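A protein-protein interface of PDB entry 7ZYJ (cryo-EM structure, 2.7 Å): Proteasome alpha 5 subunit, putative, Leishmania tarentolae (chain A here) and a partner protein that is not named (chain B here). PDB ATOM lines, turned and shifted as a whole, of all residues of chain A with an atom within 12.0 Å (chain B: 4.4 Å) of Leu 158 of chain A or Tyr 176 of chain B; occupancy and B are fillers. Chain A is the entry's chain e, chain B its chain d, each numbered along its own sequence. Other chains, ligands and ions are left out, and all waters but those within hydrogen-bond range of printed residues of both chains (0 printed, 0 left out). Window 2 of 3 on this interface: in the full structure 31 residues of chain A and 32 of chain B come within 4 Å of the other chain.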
ATOM      1  N   LYS A 152      26.714  14.516   6.883  1.00  0.00           N
ATOM      2  CA  LYS A 152      26.883  13.778   5.636  1.00  0.00           C
ATOM      3  C   LYS A 152      27.965  14.393   4.753  1.00  0.00           C
ATOM      4  O   LYS A 152      28.841  13.680   4.252  1.00  0.00           O
ATOM      5  CB  LYS A 152      25.552  13.706   4.885  1.00  0.00           C
ATOM      6  CG  LYS A 152      24.570  12.705   5.471  1.00  0.00           C
ATOM      7  CD  LYS A 152      23.233  12.753   4.754  1.00  0.00           C
ATOM      8  CE  LYS A 152      22.582  11.381   4.702  1.00  0.00           C
ATOM      9  NZ  LYS A 152      23.575  10.305   4.442  1.00  0.00           N
ATOM     10  N   ARG A 153      27.926  15.712   4.565  1.00  0.00           N
ATOM     11  CA  ARG A 153      28.849  16.429   3.682  1.00  0.00           C
ATOM     12  C   ARG A 153      28.940  15.762   2.308  1.00  0.00           C
ATOM     13  O   ARG A 153      29.991  15.276   1.888  1.00  0.00           O
ATOM     14  CB  ARG A 153      30.236  16.562   4.315  1.00  0.00           C
ATOM     15  CG  ARG A 153      30.278  17.442   5.544  1.00  0.00           C
ATOM     16  CD  ARG A 153      31.675  17.511   6.135  1.00  0.00           C
ATOM     17  NE  ARG A 153      32.612  18.188   5.247  1.00  0.00           N
ATOM     18  CZ  ARG A 153      33.922  18.246   5.446  1.00  0.00           C
ATOM     19  NH1 ARG A 153      34.487  17.680   6.498  1.00  0.00           N
ATOM     20  NH2 ARG A 153      34.684  18.889   4.566  1.00  0.00           N
ATOM     21  N   VAL A 154      27.810  15.741   1.614  1.00  0.00           N
ATOM     22  CA  VAL A 154      27.790  15.174   0.261  1.00  0.00           C
ATOM     23  C   VAL A 154      28.591  16.075  -0.671  1.00  0.00           C
ATOM     24  O   VAL A 154      28.568  17.307  -0.506  1.00  0.00           O
ATOM     25  CB  VAL A 154      26.349  15.008  -0.227  1.00  0.00           C
ATOM     26  CG1 VAL A 154      25.635  13.946   0.592  1.00  0.00           C
ATOM     27  CG2 VAL A 154      25.600  16.330  -0.148  1.00  0.00           C
ATOM     28  N   PRO A 155      29.323  15.521  -1.642  1.00  0.00           N
ATOM     29  CA  PRO A 155      30.087  16.379  -2.559  1.00  0.00           C
ATOM     30  C   PRO A 155      29.219  17.166  -3.523  1.00  0.00           C
ATOM     31  O   PRO A 155      29.687  18.176  -4.063  1.00  0.00           O
ATOM     32  CB  PRO A 155      30.987  15.385  -3.304  1.00  0.00           C
ATOM     33  CG  PRO A 155      30.253  14.091  -3.231  1.00  0.00           C
ATOM     34  CD  PRO A 155      29.528  14.089  -1.917  1.00  0.00           C
ATOM     35  N   SER A 156      27.979  16.745  -3.754  1.00  0.00           N
ATOM     36  CA  SER A 156      27.112  17.415  -4.711  1.00  0.00           C
ATOM     37  C   SER A 156      25.663  17.093  -4.380  1.00  0.00           C
ATOM     38  O   SER A 156      25.369  16.129  -3.670  1.00  0.00           O
ATOM     39  CB  SER A 156      27.440  17.000  -6.149  1.00  0.00           C
ATOM     40  OG  SER A 156      26.390  17.350  -7.032  1.00  0.00           O
ATOM     41  N   THR A 157      24.760  17.918  -4.910  1.00  0.00           N
ATOM     42  CA  THR A 157      23.332  17.692  -4.737  1.00  0.00           C
ATOM     43  C   THR A 157      22.810  16.547  -5.595  1.00  0.00           C
ATOM     44  O   THR A 157      21.680  16.096  -5.377  1.00  0.00           O
ATOM     45  CB  THR A 157      22.549  18.967  -5.063  1.00  0.00           C
ATOM     46  OG1 THR A 157      23.068  19.558  -6.260  1.00  0.00           O
ATOM     47  CG2 THR A 157      22.663  19.964  -3.922  1.00  0.00           C
ATOM     48  N   LEU A 158      23.598  16.072  -6.557  1.00  0.00           N
ATOM     49  CA  LEU A 158      23.221  14.938  -7.387  1.00  0.00           C
ATOM     50  C   LEU A 158      23.507  13.598  -6.723  1.00  0.00           C
ATOM     51  O   LEU A 158      23.064  12.563  -7.233  1.00  0.00           O
ATOM     52  CB  LEU A 158      23.953  15.007  -8.732  1.00  0.00           C
ATOM     53  CG  LEU A 158      23.602  16.204  -9.618  1.00  0.00           C
ATOM     54  CD1 LEU A 158      24.651  16.406 -10.699  1.00  0.00           C
ATOM     55  CD2 LEU A 158      22.227  16.024 -10.235  1.00  0.00           C
ATOM     56  N   VAL A 159      24.230  13.593  -5.605  1.00  0.00           N
ATOM     57  CA  VAL A 159      24.554  12.351  -4.918  1.00  0.00           C
ATOM     58  C   VAL A 159      23.321  11.834  -4.192  1.00  0.00           C
ATOM     59  O   VAL A 159      22.614  12.593  -3.517  1.00  0.00           O
ATOM     60  CB  VAL A 159      25.717  12.566  -3.938  1.00  0.00           C
ATOM     61  CG1 VAL A 159      26.152  11.242  -3.330  1.00  0.00           C
ATOM     62  CG2 VAL A 159      26.877  13.250  -4.632  1.00  0.00           C
ATOM     63  N   VAL A 160      23.056  10.539  -4.328  1.00  0.00           N
ATOM     64  CA  VAL A 160      22.016   9.888  -3.539  1.00  0.00           C
ATOM     65  C   VAL A 160      22.502   9.852  -2.094  1.00  0.00           C
ATOM     66  O   VAL A 160      23.496   9.175  -1.793  1.00  0.00           O
ATOM     67  CB  VAL A 160      21.706   8.478  -4.066  1.00  0.00           C
ATOM     68  CG1 VAL A 160      20.638   7.816  -3.214  1.00  0.00           C
ATOM     69  CG2 VAL A 160      21.270   8.545  -5.521  1.00  0.00           C
ATOM     70  N   PRO A 161      21.846  10.567  -1.176  1.00  0.00           N
ATOM     71  CA  PRO A 161      22.382  10.677   0.191  1.00  0.00           C
ATOM     72  C   PRO A 161      22.464   9.355   0.933  1.00  0.00           C
ATOM     73  O   PRO A 161      23.281   9.232   1.855  1.00  0.00           O
ATOM     74  CB  PRO A 161      21.406  11.643   0.875  1.00  0.00           C
ATOM     75  CG  PRO A 161      20.147  11.535   0.084  1.00  0.00           C
ATOM     76  CD  PRO A 161      20.565  11.275  -1.332  1.00  0.00           C
ATOM     77  N   SER A 162      21.654   8.362   0.568  1.00  0.00           N
ATOM     78  CA  SER A 162      21.697   7.071   1.240  1.00  0.00           C
ATOM     79  C   SER A 162      22.903   6.232   0.841  1.00  0.00           C
ATOM     80  O   SER A 162      23.203   5.247   1.522  1.00  0.00           O
ATOM     81  CB  SER A 162      20.412   6.289   0.958  1.00  0.00           C
ATOM     82  OG  SER A 162      20.313   5.948  -0.413  1.00  0.00           O
ATOM     83  N   SER A 163      23.598   6.595  -0.234  1.00  0.00           N
ATOM     84  CA  SER A 163      24.765   5.851  -0.689  1.00  0.00           C
ATOM     85  C   SER A 163      26.042   6.245   0.037  1.00  0.00           C
ATOM     86  O   SER A 163      27.089   5.638  -0.211  1.00  0.00           O
ATOM     87  CB  SER A 163      24.955   6.043  -2.192  1.00  0.00           C
ATOM     88  OG  SER A 163      25.285   7.386  -2.494  1.00  0.00           O
ATOM     89  N   MET A 164      25.984   7.237   0.918  1.00  0.00           N
ATOM     90  CA  MET A 164      27.126   7.683   1.708  1.00  0.00           C
ATOM     91  C   MET A 164      26.780   7.634   3.186  1.00  0.00           C
ATOM     92  O   MET A 164      27.020   8.575   3.945  1.00  0.00           O
ATOM     93  CB  MET A 164      27.566   9.084   1.298  1.00  0.00           C
ATOM     94  CG  MET A 164      28.357   9.131   0.003  1.00  0.00           C
ATOM     95  SD  MET A 164      28.543  10.809  -0.625  1.00  0.00           S
ATOM     96  CE  MET A 164      29.071  11.664   0.858  1.00  0.00           C
ATOM     97  N   ASP A 308      27.532  23.976   6.478  1.00  0.00           N
ATOM     98  CA  ASP A 308      26.322  24.011   5.675  1.00  0.00           C
ATOM     99  C   ASP A 308      25.104  24.197   6.581  1.00  0.00           C
ATOM    100  O   ASP A 308      25.193  24.137   7.810  1.00  0.00           O
ATOM    101  CB  ASP A 308      26.211  22.738   4.838  1.00  0.00           C
ATOM    102  CG  ASP A 308      25.259  22.886   3.665  1.00  0.00           C
ATOM    103  OD1 ASP A 308      24.512  23.886   3.622  1.00  0.00           O
ATOM    104  OD2 ASP A 308      25.260  22.000   2.784  1.00  0.00           O
ATOM    105  N   GLU A 313      17.757  15.890   5.316  1.00  0.00           N
ATOM    106  CA  GLU A 313      18.585  15.018   4.496  1.00  0.00           C
ATOM    107  C   GLU A 313      20.061  15.392   4.545  1.00  0.00           C
ATOM    108  O   GLU A 313      20.865  14.793   3.825  1.00  0.00           O
ATOM    109  CB  GLU A 313      18.090  15.032   3.047  1.00  0.00           C
ATOM    110  CG  GLU A 313      16.703  14.436   2.857  1.00  0.00           C
ATOM    111  CD  GLU A 313      15.592  15.427   3.152  1.00  0.00           C
ATOM    112  OE1 GLU A 313      15.901  16.605   3.427  1.00  0.00           O
ATOM    113  OE2 GLU A 313      14.410  15.026   3.114  1.00  0.00           O
ATOM    114  N   ASN A 314      20.436  16.368   5.374  1.00  0.00           N
ATOM    115  CA  ASN A 314      21.825  16.812   5.421  1.00  0.00           C
ATOM    116  C   ASN A 314      22.640  16.053   6.460  1.00  0.00           C
ATOM    117  O   ASN A 314      23.872  16.024   6.370  1.00  0.00           O
ATOM    118  CB  ASN A 314      21.887  18.313   5.704  1.00  0.00           C
ATOM    119  CG  ASN A 314      22.974  19.009   4.914  1.00  0.00           C
ATOM    120  OD1 ASN A 314      23.415  18.515   3.877  1.00  0.00           O
ATOM    121  ND2 ASN A 314      23.403  20.169   5.392  1.00  0.00           N
ATOM    122  N   VAL B  35      24.192   9.494 -16.542  1.00  0.00           N
ATOM    123  CA  VAL B  35      22.910  10.131 -16.265  1.00  0.00           C
ATOM    124  C   VAL B  35      21.886   9.052 -15.949  1.00  0.00           C
ATOM    125  O   VAL B  35      21.788   8.047 -16.661  1.00  0.00           O
ATOM    126  CB  VAL B  35      22.432  10.999 -17.448  1.00  0.00           C
ATOM    127  CG1 VAL B  35      21.142  11.718 -17.092  1.00  0.00           C
ATOM    128  CG2 VAL B  35      23.504  11.999 -17.844  1.00  0.00           C
ATOM    129  N   LEU B  36      21.121   9.264 -14.883  1.00  0.00           N
ATOM    130  CA  LEU B  36      20.089   8.335 -14.446  1.00  0.00           C
ATOM    131  C   LEU B  36      18.721   8.884 -14.821  1.00  0.00           C
ATOM    132  O   LEU B  36      18.411  10.045 -14.531  1.00  0.00           O
ATOM    133  CB  LEU B  36      20.170   8.101 -12.936  1.00  0.00           C
ATOM    134  CG  LEU B  36      19.224   7.049 -12.361  1.00  0.00           C
ATOM    135  CD1 LEU B  36      19.767   5.655 -12.613  1.00  0.00           C
ATOM    136  CD2 LEU B  36      19.007   7.283 -10.876  1.00  0.00           C
ATOM    137  N   TRP B 156      24.942   8.188  -7.686  1.00  0.00           N
ATOM    138  CA  TRP B 156      24.607   9.513  -8.179  1.00  0.00           C
ATOM    139  C   TRP B 156      23.362   9.444  -9.052  1.00  0.00           C
ATOM    140  O   TRP B 156      22.990   8.387  -9.567  1.00  0.00           O
ATOM    141  CB  TRP B 156      25.769  10.110  -8.983  1.00  0.00           C
ATOM    142  CG  TRP B 156      26.998  10.409  -8.181  1.00  0.00           C
ATOM    143  CD1 TRP B 156      27.784   9.511  -7.521  1.00  0.00           C
ATOM    144  CD2 TRP B 156      27.600  11.693  -7.980  1.00  0.00           C
ATOM    145  NE1 TRP B 156      28.829  10.157  -6.908  1.00  0.00           N
ATOM    146  CE2 TRP B 156      28.741  11.497  -7.177  1.00  0.00           C
ATOM    147  CE3 TRP B 156      27.283  12.989  -8.396  1.00  0.00           C
ATOM    148  CZ2 TRP B 156      29.565  12.548  -6.782  1.00  0.00           C
ATOM    149  CZ3 TRP B 156      28.102  14.030  -8.003  1.00  0.00           C
ATOM    150  CH2 TRP B 156      29.229  13.804  -7.205  1.00  0.00           C
ATOM    151  N   ARG B 157      22.715  10.597  -9.208  1.00  0.00           N
ATOM    152  CA  ARG B 157      21.711  10.779 -10.247  1.00  0.00           C
ATOM    153  C   ARG B 157      22.318  11.286 -11.544  1.00  0.00           C
ATOM    154  O   ARG B 157      21.791  10.998 -12.622  1.00  0.00           O
ATOM    155  CB  ARG B 157      20.628  11.754  -9.777  1.00  0.00           C
ATOM    156  CG  ARG B 157      19.585  11.127  -8.869  1.00  0.00           C
ATOM    157  CD  ARG B 157      18.730  12.187  -8.198  1.00  0.00           C
ATOM    158  NE  ARG B 157      19.500  13.377  -7.859  1.00  0.00           N
ATOM    159  CZ  ARG B 157      19.016  14.610  -7.868  1.00  0.00           C
ATOM    160  NH1 ARG B 157      17.758  14.856  -8.195  1.00  0.00           N
ATOM    161  NH2 ARG B 157      19.812  15.623  -7.541  1.00  0.00           N
ATOM    162  N   ALA B 158      23.417  12.030 -11.447  1.00  0.00           N
ATOM    163  CA  ALA B 158      24.209  12.438 -12.598  1.00  0.00           C
ATOM    164  C   ALA B 158      25.630  12.666 -12.108  1.00  0.00           C
ATOM    165  O   ALA B 158      25.844  13.443 -11.175  1.00  0.00           O
ATOM    166  CB  ALA B 158      23.646  13.706 -13.248  1.00  0.00           C
ATOM    167  N   ILE B 169      29.961  18.604 -13.284  1.00  0.00           N
ATOM    168  CA  ILE B 169      29.051  18.306 -12.182  1.00  0.00           C
ATOM    169  C   ILE B 169      28.332  19.569 -11.730  1.00  0.00           C
ATOM    170  O   ILE B 169      27.110  19.572 -11.535  1.00  0.00           O
ATOM    171  CB  ILE B 169      29.815  17.643 -11.022  1.00  0.00           C
ATOM    172  CG1 ILE B 169      30.241  16.225 -11.405  1.00  0.00           C
ATOM    173  CG2 ILE B 169      28.965  17.625  -9.763  1.00  0.00           C
ATOM    174  CD1 ILE B 169      30.875  15.449 -10.274  1.00  0.00           C
ATOM    175  N   MET B 172      25.663  20.559 -14.430  1.00  0.00           N
ATOM    176  CA  MET B 172      24.448  19.754 -14.488  1.00  0.00           C
ATOM    177  C   MET B 172      23.753  19.630 -13.138  1.00  0.00           C
ATOM    178  O   MET B 172      22.686  19.013 -13.066  1.00  0.00           O
ATOM    179  CB  MET B 172      24.746  18.362 -15.053  1.00  0.00           C
ATOM    180  CG  MET B 172      25.820  17.587 -14.331  1.00  0.00           C
ATOM    181  SD  MET B 172      26.218  16.051 -15.185  1.00  0.00           S
ATOM    182  CE  MET B 172      27.133  15.193 -13.911  1.00  0.00           C
ATOM    183  N   GLU B 173      24.323  20.194 -12.071  1.00  0.00           N
ATOM    184  CA  GLU B 173      23.581  20.286 -10.819  1.00  0.00           C
ATOM    185  C   GLU B 173      22.367  21.195 -10.952  1.00  0.00           C
ATOM    186  O   GLU B 173      21.320  20.921 -10.354  1.00  0.00           O
ATOM    187  CB  GLU B 173      24.489  20.791  -9.699  1.00  0.00           C
ATOM    188  CG  GLU B 173      25.248  19.703  -8.965  1.00  0.00           C
ATOM    189  CD  GLU B 173      26.156  20.259  -7.887  1.00  0.00           C
ATOM    190  OE1 GLU B 173      25.635  20.763  -6.870  1.00  0.00           O
ATOM    191  OE2 GLU B 173      27.391  20.193  -8.056  1.00  0.00           O
ATOM    192  N   LYS B 174      22.486  22.272 -11.726  1.00  0.00           N
ATOM    193  CA  LYS B 174      21.434  23.268 -11.863  1.00  0.00           C
ATOM    194  C   LYS B 174      20.534  23.021 -13.067  1.00  0.00           C
ATOM    195  O   LYS B 174      19.635  23.827 -13.329  1.00  0.00           O
ATOM    196  CB  LYS B 174      22.049  24.665 -11.958  1.00  0.00           C
ATOM    197  CG  LYS B 174      22.778  24.928 -13.266  1.00  0.00           C
ATOM    198  CD  LYS B 174      23.431  26.299 -13.274  1.00  0.00           C
ATOM    199  CE  LYS B 174      24.405  26.451 -12.118  1.00  0.00           C
ATOM    200  NZ  LYS B 174      25.527  25.477 -12.209  1.00  0.00           N
ATOM    201  N   SER B 175      20.747  21.930 -13.806  1.00  0.00           N
ATOM    202  CA  SER B 175      19.963  21.687 -15.011  1.00  0.00           C
ATOM    203  C   SER B 175      19.459  20.253 -15.123  1.00  0.00           C
ATOM    204  O   SER B 175      18.813  19.922 -16.126  1.00  0.00           O
ATOM    205  CB  SER B 175      20.779  22.041 -16.260  1.00  0.00           C
ATOM    206  OG  SER B 175      21.893  21.177 -16.404  1.00  0.00           O
ATOM    207  N   TYR B 176      19.722  19.395 -14.142  1.00  0.00           N
ATOM    208  CA  TYR B 176      19.271  18.010 -14.187  1.00  0.00           C
ATOM    209  C   TYR B 176      17.872  17.925 -13.591  1.00  0.00           C
ATOM    210  O   TYR B 176      17.635  18.407 -12.478  1.00  0.00           O
ATOM    211  CB  TYR B 176      20.238  17.096 -13.435  1.00  0.00           C
ATOM    212  CG  TYR B 176      19.690  15.718 -13.127  1.00  0.00           C
ATOM    213  CD1 TYR B 176      19.799  14.687 -14.051  1.00  0.00           C
ATOM    214  CD2 TYR B 176      19.081  15.443 -11.909  1.00  0.00           C
ATOM    215  CE1 TYR B 176      19.305  13.427 -13.777  1.00  0.00           C
ATOM    216  CE2 TYR B 176      18.584  14.187 -11.627  1.00  0.00           C
ATOM    217  CZ  TYR B 176      18.700  13.183 -12.564  1.00  0.00           C
ATOM    218  OH  TYR B 176      18.208  11.928 -12.287  1.00  0.00           O
ATOM    219  N   LYS B 177      16.953  17.312 -14.327  1.00  0.00           N
ATOM    220  CA  LYS B 177      15.589  17.111 -13.864  1.00  0.00           C
ATOM    221  C   LYS B 177      15.380  15.647 -13.505  1.00  0.00           C
ATOM    222  O   LYS B 177      15.898  14.751 -14.176  1.00  0.00           O
ATOM    223  CB  LYS B 177      14.575  17.544 -14.927  1.00  0.00           C
ATOM    224  CG  LYS B 177      14.587  19.036 -15.246  1.00  0.00           C
ATOM    225  CD  LYS B 177      14.855  19.893 -14.015  1.00  0.00           C
ATOM    226  CE  LYS B 177      13.644  19.950 -13.091  1.00  0.00           C
ATOM    227  NZ  LYS B 177      13.908  20.785 -11.886  1.00  0.00           N
ATOM    228  N   ASP B 178      14.634  15.411 -12.430  1.00  0.00           N
ATOM    229  CA  ASP B 178      14.375  14.048 -11.991  1.00  0.00           C
ATOM    230  C   ASP B 178      13.396  13.358 -12.933  1.00  0.00           C
ATOM    231  O   ASP B 178      12.441  13.969 -13.421  1.00  0.00           O
ATOM    232  CB  ASP B 178      13.827  14.049 -10.565  1.00  0.00           C
ATOM    233  CG  ASP B 178      13.842  12.671  -9.934  1.00  0.00           C
ATOM    234  OD1 ASP B 178      13.057  11.803 -10.370  1.00  0.00           O
ATOM    235  OD2 ASP B 178      14.642  12.455  -8.999  1.00  0.00           O
ATOM    236  N   PHE B 188      20.568  14.946 -22.482  1.00  0.00           N
ATOM    237  CA  PHE B 188      21.190  15.585 -21.328  1.00  0.00           C
ATOM    238  C   PHE B 188      22.662  15.212 -21.197  1.00  0.00           C
ATOM    239  O   PHE B 188      23.489  16.062 -20.848  1.00  0.00           O
ATOM    240  CB  PHE B 188      20.436  15.214 -20.052  1.00  0.00           C
ATOM    241  CG  PHE B 188      20.917  15.946 -18.835  1.00  0.00           C
ATOM    242  CD1 PHE B 188      20.527  17.253 -18.600  1.00  0.00           C
ATOM    243  CD2 PHE B 188      21.763  15.330 -17.929  1.00  0.00           C
ATOM    244  CE1 PHE B 188      20.969  17.931 -17.483  1.00  0.00           C
ATOM    245  CE2 PHE B 188      22.208  16.004 -16.811  1.00  0.00           C
ATOM    246  CZ  PHE B 188      21.811  17.305 -16.588  1.00  0.00           C
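Among the printed residues, pairs that only touch across the chains: Leu 158 of chain A with Ala 158 of chain B, Val 159 of chain A with Trp 156 of chain B, Leu 158 of chain A with Trp 156 of chain B, Ser 156 of chain A with Trp 156 of chain B, Leu 158 of chain A with Tyr 176 of chain B, Ser 156 of chain A with Ile 169 of chain B, Leu 158 of chain A with Glu 173 of chain B, Pro 155 of chain A with Trp 156 of chain B and Leu 158 of chain A with Met 172 of chain B.
Printed residues of chain B within 4 Å of Leu 158 of chain A: Trp 156 (3.5 Å), Arg 157 (2.8 Å), Ala 158 (3.2 Å), Met 172 (3.99 Å), Glu 173 (3.8 Å) and Tyr 176 (3.6 Å).
Of chain A, only Leu 158 comes within 4 Å of Tyr 176 of chain B.
No residue of chain A comes within 4 Å of Val 35 of chain B.
No residue of chain A comes within 4 Å of Leu 36 of chain B.
Of the printed residues of chain A, Trp 156 of chain B touches Pro 155, Ser 156, Leu 158 and Val 159.
Arg 157 of chain B touches just these residues of chain A: Thr 157 and Leu 158.
Glu 173 of chain B touches three residues of chain A.
No residue of chain A comes within 4 Å of Ser 175 of chain B.
No residue of chain A comes within 4 Å of Lys 177 of chain B.
No residue of chain A comes within 4 Å of Asp 178 of chain B.
Of the printed residues of chain B, Thr 157 of chain A touches Arg 157 and Glu 173.
Of the printed residues of chain A, Met 172 of chain B touches Leu 158.
Printed residues of chain B within 4 Å of Ser 156 of chain A: Trp 156 (3.6 Å), Ile 169 (3.8 Å) and Glu 173 (3.0 Å).
Of the printed residues of chain B, Val 159 of chain A touches Trp 156 (3.5 Å).
Arg 153 of chain A touches none of the printed residues of chain B.
The nearest residue of chain A that does not touch Tyr 176 of chain B is Thr 157 of chain A (7.1 Å).
The nearest printed residue of chain A that does not touch Met 172 of chain B is Thr 157 of chain A (6.8 Å).
Hydrophobic or aromatic side chains of chain B that line the printed part of chain A: Trp 156, Ala 158, Ile 169, Met 172 and Tyr 176.
Printed residues of chain A that touch a printed residue of chain B: Pro 155, Ser 156, Thr 157, Leu 158 and Val 159.
Hydrophobic or aromatic side chains of chain A within 4 Å of the printed part of chain B: Pro 155, Leu 158 and Val 159.
Among the printed residues, 13 pairs touch across the chains.
NH2 of Arg 157 of chain B lies within hydrogen-bond range of O of Thr 157 of chain A (2.9 Å).
O of Leu 158 of chain A lies within hydrogen-bond range of N of Arg 157 of chain B (2.8 Å).
OG of Ser 156 of chain A lies close to OE2 of Glu 173 of chain B, 3.2 Å away.
The side-chain hydroxyl (OG1) of Thr 157 of chain A lies within hydrogen-bond range of the side-chain carboxylate (OE1) of Glu 173 of chain B (2.9 Å).
The backbone carbonyl oxygen (O) of Arg 157 of chain B sits at hydrogen-bond distance from the backbone NH (N) of Leu 36 of chain B.
The backbone carbonyl oxygen (O) of Leu 36 of chain B is in hydrogen-bond range of the side-chain hydroxyl (OH) of Tyr 176 of chain B, 2.9 Å away.
The side-chain hydroxyl of Ser 156 of chain A lies within hydrogen-bond range of the backbone NH of Leu 158 of chain A.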
